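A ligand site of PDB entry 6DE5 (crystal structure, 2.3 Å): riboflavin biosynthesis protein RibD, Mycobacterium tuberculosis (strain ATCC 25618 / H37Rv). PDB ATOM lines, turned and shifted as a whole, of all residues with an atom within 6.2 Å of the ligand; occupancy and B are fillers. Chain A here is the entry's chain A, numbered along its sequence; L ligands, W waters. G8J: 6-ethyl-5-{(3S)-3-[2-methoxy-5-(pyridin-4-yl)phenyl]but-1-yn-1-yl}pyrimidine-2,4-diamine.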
ATOM      1  N   ASN A  44       0.077  10.484  -1.189  1.00  0.00           N
ATOM      2  CA  ASN A  44       1.084   9.619  -0.607  1.00  0.00           C
ATOM      3  C   ASN A  44       0.843   8.204  -1.071  1.00  0.00           C
ATOM      4  O   ASN A  44      -0.205   7.640  -0.791  1.00  0.00           O
ATOM      5  CB  ASN A  44       1.079   9.692   0.914  1.00  0.00           C
ATOM      6  CG  ASN A  44       2.195   8.857   1.546  1.00  0.00           C
ATOM      7  OD1 ASN A  44       3.278   8.679   0.961  1.00  0.00           O
ATOM      8  ND2 ASN A  44       1.937   8.330   2.748  1.00  0.00           N
ATOM      9  N   PHE A  45       1.767   7.651  -1.825  1.00  0.00           N
ATOM     10  CA  PHE A  45       1.669   6.241  -2.196  1.00  0.00           C
ATOM     11  C   PHE A  45       2.966   5.494  -1.889  1.00  0.00           C
ATOM     12  O   PHE A  45       3.983   6.131  -1.602  1.00  0.00           O
ATOM     13  CB  PHE A  45       1.276   6.104  -3.660  1.00  0.00           C
ATOM     14  CG  PHE A  45      -0.188   6.383  -3.909  1.00  0.00           C
ATOM     15  CD1 PHE A  45      -0.684   7.675  -3.805  1.00  0.00           C
ATOM     16  CD2 PHE A  45      -1.064   5.345  -4.188  1.00  0.00           C
ATOM     17  CE1 PHE A  45      -2.039   7.947  -3.983  1.00  0.00           C
ATOM     18  CE2 PHE A  45      -2.427   5.606  -4.383  1.00  0.00           C
ATOM     19  CZ  PHE A  45      -2.912   6.916  -4.275  1.00  0.00           C
ATOM     20  N   ILE A  46       2.902   4.165  -1.898  1.00  0.00           N
ATOM     21  CA  ILE A  46       4.089   3.311  -1.778  1.00  0.00           C
ATOM     22  C   ILE A  46       4.153   2.312  -2.956  1.00  0.00           C
ATOM     23  O   ILE A  46       3.131   1.823  -3.441  1.00  0.00           O
ATOM     24  CB  ILE A  46       4.134   2.536  -0.427  1.00  0.00           C
ATOM     25  CG1 ILE A  46       5.436   1.719  -0.317  1.00  0.00           C
ATOM     26  CG2 ILE A  46       2.908   1.638  -0.262  1.00  0.00           C
ATOM     27  CD1 ILE A  46       5.672   1.086   1.033  1.00  0.00           C
ATOM     28  N   THR A  58      -2.848  -6.191  -0.348  1.00  0.00           N
ATOM     29  CA  THR A  58      -2.444  -5.192   0.636  1.00  0.00           C
ATOM     30  C   THR A  58      -1.311  -4.319   0.054  1.00  0.00           C
ATOM     31  O   THR A  58      -0.672  -4.695  -0.936  1.00  0.00           O
ATOM     32  CB  THR A  58      -1.998  -5.869   1.974  1.00  0.00           C
ATOM     33  OG1 THR A  58      -2.145  -4.953   3.069  1.00  0.00           O
ATOM     34  CG2 THR A  58      -0.553  -6.368   1.900  1.00  0.00           C
ATOM     35  N   SER A  59      -1.095  -3.144   0.623  1.00  0.00           N
ATOM     36  CA  SER A  59       0.124  -2.382   0.354  1.00  0.00           C
ATOM     37  C   SER A  59       0.965  -2.306   1.633  1.00  0.00           C
ATOM     38  O   SER A  59       2.095  -1.790   1.626  1.00  0.00           O
ATOM     39  CB  SER A  59      -0.210  -0.987  -0.187  1.00  0.00           C
ATOM     40  OG  SER A  59      -1.242  -0.370   0.563  1.00  0.00           O
ATOM     41  N   GLY A  60       0.385  -2.833   2.721  1.00  0.00           N
ATOM     42  CA  GLY A  60       1.002  -2.851   4.030  1.00  0.00           C
ATOM     43  C   GLY A  60       2.220  -3.760   4.158  1.00  0.00           C
ATOM     44  O   GLY A  60       3.063  -3.539   5.032  1.00  0.00           O
ATOM     45  N   ALA A  63       5.361  -1.864   3.451  1.00  0.00           N
ATOM     46  CA  ALA A  63       5.545  -0.764   4.377  1.00  0.00           C
ATOM     47  C   ALA A  63       6.212  -1.205   5.669  1.00  0.00           C
ATOM     48  O   ALA A  63       5.644  -1.992   6.402  1.00  0.00           O
ATOM     49  CB  ALA A  63       4.202  -0.118   4.675  1.00  0.00           C
ATOM     50  N   ASP A  67       8.192   3.887   6.524  1.00  0.00           N
ATOM     51  CA  ASP A  67       7.053   4.303   5.745  1.00  0.00           C
ATOM     52  C   ASP A  67       5.843   4.637   6.633  1.00  0.00           C
ATOM     53  O   ASP A  67       5.163   5.648   6.417  1.00  0.00           O
ATOM     54  CB  ASP A  67       6.677   3.236   4.745  1.00  0.00           C
ATOM     55  CG  ASP A  67       5.588   3.671   3.797  1.00  0.00           C
ATOM     56  OD1 ASP A  67       5.708   4.764   3.175  1.00  0.00           O
ATOM     57  OD2 ASP A  67       4.610   2.927   3.673  1.00  0.00           O
ATOM     58  N   ARG A  68       5.569   3.796   7.608  1.00  0.00           N
ATOM     59  CA  ARG A  68       4.447   4.028   8.507  1.00  0.00           C
ATOM     60  C   ARG A  68       4.552   5.389   9.209  1.00  0.00           C
ATOM     61  O   ARG A  68       3.575   6.112   9.309  1.00  0.00           O
ATOM     62  CB  ARG A  68       4.372   2.923   9.556  1.00  0.00           C
ATOM     63  CG  ARG A  68       3.923   1.590   9.011  1.00  0.00           C
ATOM     64  CD  ARG A  68       3.686   0.620  10.177  1.00  0.00           C
ATOM     65  NE  ARG A  68       2.934  -0.532   9.710  1.00  0.00           N
ATOM     66  CZ  ARG A  68       2.040  -1.202  10.429  1.00  0.00           C
ATOM     67  NH1 ARG A  68       1.776  -0.832  11.673  1.00  0.00           N
ATOM     68  NH2 ARG A  68       1.415  -2.228   9.880  1.00  0.00           N
ATOM     69  N   PHE A  71       3.869   8.032   6.832  1.00  0.00           N
ATOM     70  CA  PHE A  71       2.445   7.891   6.533  1.00  0.00           C
ATOM     71  C   PHE A  71       1.567   8.576   7.598  1.00  0.00           C
ATOM     72  O   PHE A  71       0.660   9.329   7.265  1.00  0.00           O
ATOM     73  CB  PHE A  71       2.079   6.394   6.410  1.00  0.00           C
ATOM     74  CG  PHE A  71       0.646   6.140   6.052  1.00  0.00           C
ATOM     75  CD1 PHE A  71      -0.322   6.003   7.038  1.00  0.00           C
ATOM     76  CD2 PHE A  71       0.264   6.034   4.715  1.00  0.00           C
ATOM     77  CE1 PHE A  71      -1.665   5.787   6.713  1.00  0.00           C
ATOM     78  CE2 PHE A  71      -1.081   5.811   4.378  1.00  0.00           C
ATOM     79  CZ  PHE A  71      -2.043   5.679   5.393  1.00  0.00           C
ATOM     80  N   ASN A  72       1.862   8.319   8.879  1.00  0.00           N
ATOM     81  CA  ASN A  72       1.076   8.931   9.939  1.00  0.00           C
ATOM     82  C   ASN A  72       1.350  10.420  10.046  1.00  0.00           C
ATOM     83  O   ASN A  72       0.427  11.197  10.264  1.00  0.00           O
ATOM     84  CB  ASN A  72       1.345   8.250  11.286  1.00  0.00           C
ATOM     85  CG  ASN A  72       0.900   6.810  11.294  1.00  0.00           C
ATOM     86  OD1 ASN A  72      -0.230   6.498  10.945  1.00  0.00           O
ATOM     87  ND2 ASN A  72       1.822   5.912  11.630  1.00  0.00           N
ATOM     88  N   ARG A  75      -0.630  12.276   7.583  1.00  0.00           N
ATOM     89  CA  ARG A  75      -2.011  12.358   8.079  1.00  0.00           C
ATOM     90  C   ARG A  75      -2.163  13.447   9.123  1.00  0.00           C
ATOM     91  O   ARG A  75      -3.154  14.170   9.137  1.00  0.00           O
ATOM     92  CB  ARG A  75      -2.472  11.024   8.661  1.00  0.00           C
ATOM     93  CG  ARG A  75      -3.004  10.088   7.619  1.00  0.00           C
ATOM     94  CD  ARG A  75      -3.493   8.784   8.236  1.00  0.00           C
ATOM     95  NE  ARG A  75      -4.167   7.981   7.214  1.00  0.00           N
ATOM     96  CZ  ARG A  75      -5.188   7.165   7.439  1.00  0.00           C
ATOM     97  NH1 ARG A  75      -5.643   7.002   8.674  1.00  0.00           N
ATOM     98  NH2 ARG A  75      -5.729   6.499   6.425  1.00  0.00           N
ATOM     99  N   THR A  87     -11.192   1.489  -1.772  1.00  0.00           N
ATOM    100  CA  THR A  87     -10.169   1.339  -0.740  1.00  0.00           C
ATOM    101  C   THR A  87     -10.784   1.228   0.655  1.00  0.00           C
ATOM    102  O   THR A  87     -10.358   0.417   1.488  1.00  0.00           O
ATOM    103  CB  THR A  87      -9.178   2.506  -0.793  1.00  0.00           C
ATOM    104  OG1 THR A  87      -8.301   2.335  -1.911  1.00  0.00           O
ATOM    105  CG2 THR A  87      -8.343   2.600   0.479  1.00  0.00           C
ATOM    106  N   ILE A  90     -11.881  -2.155   2.007  1.00  0.00           N
ATOM    107  CA  ILE A  90     -10.894  -3.228   2.098  1.00  0.00           C
ATOM    108  C   ILE A  90     -10.650  -3.602   3.567  1.00  0.00           C
ATOM    109  O   ILE A  90     -10.680  -2.746   4.471  1.00  0.00           O
ATOM    110  CB  ILE A  90      -9.574  -2.839   1.386  1.00  0.00           C
ATOM    111  CG1 ILE A  90      -9.830  -2.301  -0.023  1.00  0.00           C
ATOM    112  CG2 ILE A  90      -8.748  -4.023   1.153  1.00  0.00           C
ATOM    113  CD1 ILE A  90     -10.695  -3.196  -0.941  1.00  0.00           C
ATOM    114  N   GLU A  91     -10.373  -4.895   3.780  1.00  0.00           N
ATOM    115  CA  GLU A  91     -10.383  -5.606   5.064  1.00  0.00           C
ATOM    116  C   GLU A  91     -10.262  -4.826   6.398  1.00  0.00           C
ATOM    117  O   GLU A  91     -11.069  -5.018   7.313  1.00  0.00           O
ATOM    118  CB  GLU A  91      -9.282  -6.681   5.012  1.00  0.00           C
ATOM    119  CG  GLU A  91      -7.784  -6.308   5.421  1.00  0.00           C
ATOM    120  CD  GLU A  91      -7.225  -5.004   4.843  1.00  0.00           C
ATOM    121  OE1 GLU A  91      -7.629  -4.629   3.722  1.00  0.00           O
ATOM    122  OE2 GLU A  91      -6.372  -4.357   5.499  1.00  0.00           O
ATOM    123  N   GLY A  92      -9.257  -3.957   6.517  1.00  0.00           N
ATOM    124  CA  GLY A  92      -8.876  -3.397   7.799  1.00  0.00           C
ATOM    125  C   GLY A  92      -8.542  -1.947   7.630  1.00  0.00           C
ATOM    126  O   GLY A  92      -7.540  -1.460   8.152  1.00  0.00           O
ATOM    127  N   TYR A  93      -9.388  -1.252   6.862  1.00  0.00           N
ATOM    128  CA  TYR A  93      -9.306   0.194   6.734  1.00  0.00           C
ATOM    129  C   TYR A  93     -10.029   0.864   7.892  1.00  0.00           C
ATOM    130  O   TYR A  93     -11.263   0.929   7.920  1.00  0.00           O
ATOM    131  CB  TYR A  93      -9.906   0.651   5.401  1.00  0.00           C
ATOM    132  CG  TYR A  93      -9.639   2.103   5.118  1.00  0.00           C
ATOM    133  CD1 TYR A  93      -8.506   2.498   4.418  1.00  0.00           C
ATOM    134  CD2 TYR A  93     -10.504   3.099   5.575  1.00  0.00           C
ATOM    135  CE1 TYR A  93      -8.242   3.831   4.182  1.00  0.00           C
ATOM    136  CE2 TYR A  93     -10.261   4.424   5.339  1.00  0.00           C
ATOM    137  CZ  TYR A  93      -9.125   4.788   4.646  1.00  0.00           C
ATOM    138  OH  TYR A  93      -8.902   6.127   4.405  1.00  0.00           O
ATOM    139  N   SER A  94      -9.252   1.371   8.848  1.00  0.00           N
ATOM    140  CA  SER A  94      -9.807   1.928  10.078  1.00  0.00           C
ATOM    141  C   SER A  94     -10.391   3.324   9.856  1.00  0.00           C
ATOM    142  O   SER A  94     -10.533   3.781   8.724  1.00  0.00           O
ATOM    143  CB  SER A  94      -8.727   1.987  11.160  1.00  0.00           C
ATOM    144  OG  SER A  94      -8.195   0.703  11.410  1.00  0.00           O
ATOM    145  N   THR A 192      -4.410  12.345  -0.141  1.00  0.00           N
ATOM    146  CA  THR A 192      -5.052  11.147  -0.694  1.00  0.00           C
ATOM    147  C   THR A 192      -4.077   9.981  -0.593  1.00  0.00           C
ATOM    148  O   THR A 192      -2.866  10.156  -0.737  1.00  0.00           O
ATOM    149  CB  THR A 192      -5.501  11.369  -2.171  1.00  0.00           C
ATOM    150  OG1 THR A 192      -6.321  10.275  -2.612  1.00  0.00           O
ATOM    151  CG2 THR A 192      -4.301  11.499  -3.109  1.00  0.00           C
ATOM    152  N   GLU A 193      -4.591   8.783  -0.293  1.00  0.00           N
ATOM    153  CA  GLU A 193      -3.749   7.617  -0.064  1.00  0.00           C
ATOM    154  C   GLU A 193      -4.205   6.429  -0.910  1.00  0.00           C
ATOM    155  O   GLU A 193      -3.659   5.329  -0.775  1.00  0.00           O
ATOM    156  CB  GLU A 193      -3.772   7.222   1.425  1.00  0.00           C
ATOM    157  CG  GLU A 193      -3.234   8.293   2.354  1.00  0.00           C
ATOM    158  CD  GLU A 193      -3.655   8.075   3.815  1.00  0.00           C
ATOM    159  OE1 GLU A 193      -4.633   7.342   4.055  1.00  0.00           O
ATOM    160  OE2 GLU A 193      -3.009   8.654   4.709  1.00  0.00           O
ATOM    161  N   GLY A 194      -5.192   6.660  -1.779  1.00  0.00           N
ATOM    162  CA  GLY A 194      -5.706   5.617  -2.646  1.00  0.00           C
ATOM    163  C   GLY A 194      -7.214   5.669  -2.819  1.00  0.00           C
ATOM    164  O   GLY A 194      -7.889   6.498  -2.200  1.00  0.00           O
ATOM    165  N   CYS A 212       3.971  12.189  -3.053  1.00  0.00           N
ATOM    166  CA  CYS A 212       4.890  11.621  -2.079  1.00  0.00           C
ATOM    167  C   CYS A 212       4.928  10.126  -2.293  1.00  0.00           C
ATOM    168  O   CYS A 212       3.937   9.428  -2.069  1.00  0.00           O
ATOM    169  CB  CYS A 212       4.463  11.939  -0.643  1.00  0.00           C
ATOM    170  SG  CYS A 212       4.809  13.607  -0.076  1.00  0.00           S
ATOM    171  N   LEU A 213       6.070   9.636  -2.721  1.00  0.00           N
ATOM    172  CA  LEU A 213       6.222   8.230  -3.109  1.00  0.00           C
ATOM    173  C   LEU A 213       7.281   7.548  -2.260  1.00  0.00           C
ATOM    174  O   LEU A 213       8.428   8.011  -2.194  1.00  0.00           O
ATOM    175  CB  LEU A 213       6.598   8.129  -4.589  1.00  0.00           C
ATOM    176  CG  LEU A 213       6.608   6.738  -5.224  1.00  0.00           C
ATOM    177  CD1 LEU A 213       5.212   6.131  -5.320  1.00  0.00           C
ATOM    178  CD2 LEU A 213       7.258   6.793  -6.594  1.00  0.00           C
ATOM    179  N   THR A 214       6.910   6.450  -1.621  1.00  0.00           N
ATOM    180  CA  THR A 214       7.876   5.559  -0.989  1.00  0.00           C
ATOM    181  C   THR A 214       8.281   4.472  -1.985  1.00  0.00           C
ATOM    182  O   THR A 214       7.427   3.808  -2.600  1.00  0.00           O
ATOM    183  CB  THR A 214       7.352   4.912   0.316  1.00  0.00           C
ATOM    184  OG1 THR A 214       7.151   5.914   1.316  1.00  0.00           O
ATOM    185  CG2 THR A 214       8.364   3.942   0.872  1.00  0.00           C
HETATM  186  C4  G8J L   1       1.179   3.188   2.710  1.00  0.00           C
HETATM  187  C5  G8J L   1       0.098   3.643   1.991  1.00  0.00           C
HETATM  188  C6  G8J L   1       0.289   4.737   1.119  1.00  0.00           C
HETATM  189  N1  G8J L   1       1.497   5.313   1.006  1.00  0.00           N
HETATM  190  N3  G8J L   1       2.351   3.799   2.550  1.00  0.00           N
HETATM  191  CAJ G8J L   1       1.424   2.581   5.009  1.00  0.00           C
HETATM  192  CAI G8J L   1       1.063   2.108   3.598  1.00  0.00           C
HETATM  193  C2  G8J L   1       2.529   4.836   1.717  1.00  0.00           C
HETATM  194  NAG G8J L   1       3.738   5.396   1.620  1.00  0.00           N
HETATM  195  NAH G8J L   1      -0.768   5.192   0.430  1.00  0.00           N
HETATM  196  CAK G8J L   1      -1.156   3.006   2.159  1.00  0.00           C
HETATM  197  CAL G8J L   1      -2.156   2.514   2.283  1.00  0.00           C
HETATM  198  CAM G8J L   1      -3.498   1.935   2.398  1.00  0.00           C
HETATM  199  CAZ G8J L   1      -4.496   3.081   2.247  1.00  0.00           C
HETATM  200  CAN G8J L   1      -3.675   1.307   3.642  1.00  0.00           C
HETATM  201  CAO G8J L   1      -2.798   1.564   4.710  1.00  0.00           C
HETATM  202  CAS G8J L   1      -4.734   0.423   3.827  1.00  0.00           C
HETATM  203  OBA G8J L   1      -5.566   0.212   2.746  1.00  0.00           O
HETATM  204  CBB G8J L   1      -6.560  -0.777   3.051  1.00  0.00           C
HETATM  205  CAR G8J L   1      -4.923  -0.208   5.051  1.00  0.00           C
HETATM  206  CAQ G8J L   1      -4.041   0.063   6.094  1.00  0.00           C
HETATM  207  CAP G8J L   1      -2.972   0.943   5.943  1.00  0.00           C
HETATM  208  CAT G8J L   1      -2.109   1.159   7.033  1.00  0.00           C
HETATM  209  CAU G8J L   1      -1.393   2.346   7.189  1.00  0.00           C
HETATM  210  CAV G8J L   1      -0.536   2.527   8.283  1.00  0.00           C
HETATM  211  NAW G8J L   1      -0.375   1.506   9.251  1.00  0.00           N
HETATM  212  CAX G8J L   1      -1.079   0.300   9.096  1.00  0.00           C
HETATM  213  CAY G8J L   1      -1.925   0.153   7.990  1.00  0.00           C
HETATM  214  O   HOH W   1       4.655   7.359   3.891  1.00  0.00           O
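The side-chain carboxylate (OD1) of Asp 67 sits at hydrogen-bond distance from the side-chain hydroxyl (OG1) of Thr 214 (2.6 Å). OD1 of Asn 44 lies close to O of Cys 212 (3.2 Å). N of Asn 44 sits at hydrogen-bond distance from O of Thr 192, at 3.0 Å. OE1 of Glu 193 is in salt-bridge range of NH2 of Arg 75 (2.7 Å). N of Thr 214 sits at hydrogen-bond distance from O of Phe 45, 2.9 Å away. The backbone NH of Phe 45 sits at hydrogen-bond distance from the backbone carbonyl oxygen of Cys 212. The side-chain amide nitrogen (ND2) of Asn 72 is in hydrogen-bond range of the backbone carbonyl oxygen (O) of Arg 68 (2.9 Å).
OG of Ser 59 touches CAL of the ligand (3.5 Å). Ala 63 touches the ligand (CB to CAJ, 3.9 Å). NH2 of Arg 68 touches CAX of the ligand, 3.6 Å away. Phe 71 touches the ligand (CE2 to C5, 3.4 Å). Hydrophobic or aromatic side chains that line the ligand: Ile 46, Ala 63 and Phe 71. Within 4 Å of the ligand: Asn 44, Phe 45, Ile 46, Ser 59, Ala 63, Asp 67, Arg 68, Phe 71, Glu 193 and Thr 214. Along chain A the residues within 4 Å of the ligand span positions 44 to 214.
OD1 of Asp 67 lies within hydrogen-bond range of NAG of the ligand, 2.6 Å away. The backbone carbonyl oxygen of Asn 44 lies within hydrogen-bond range of a nitrogen (NAH) of the ligand (2.8 Å). The side-chain amide oxygen of Asn 44 is in hydrogen-bond range of a nitrogen (NAG) of the ligand, 3.4 Å away. A nitrogen (NAH) of the ligand is in hydrogen-bond range of the backbone carbonyl oxygen of Glu 193. The backbone carbonyl oxygen (O) of Phe 45 lies within hydrogen-bond range of a nitrogen (NAG) of the ligand (3.3 Å). The backbone NH (N) of Ile 46 sits at hydrogen-bond distance from a nitrogen (N1) of the ligand (3.4 Å). OG1 of Thr 214 sits at hydrogen-bond distance from NAG of the ligand (3.5 Å).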
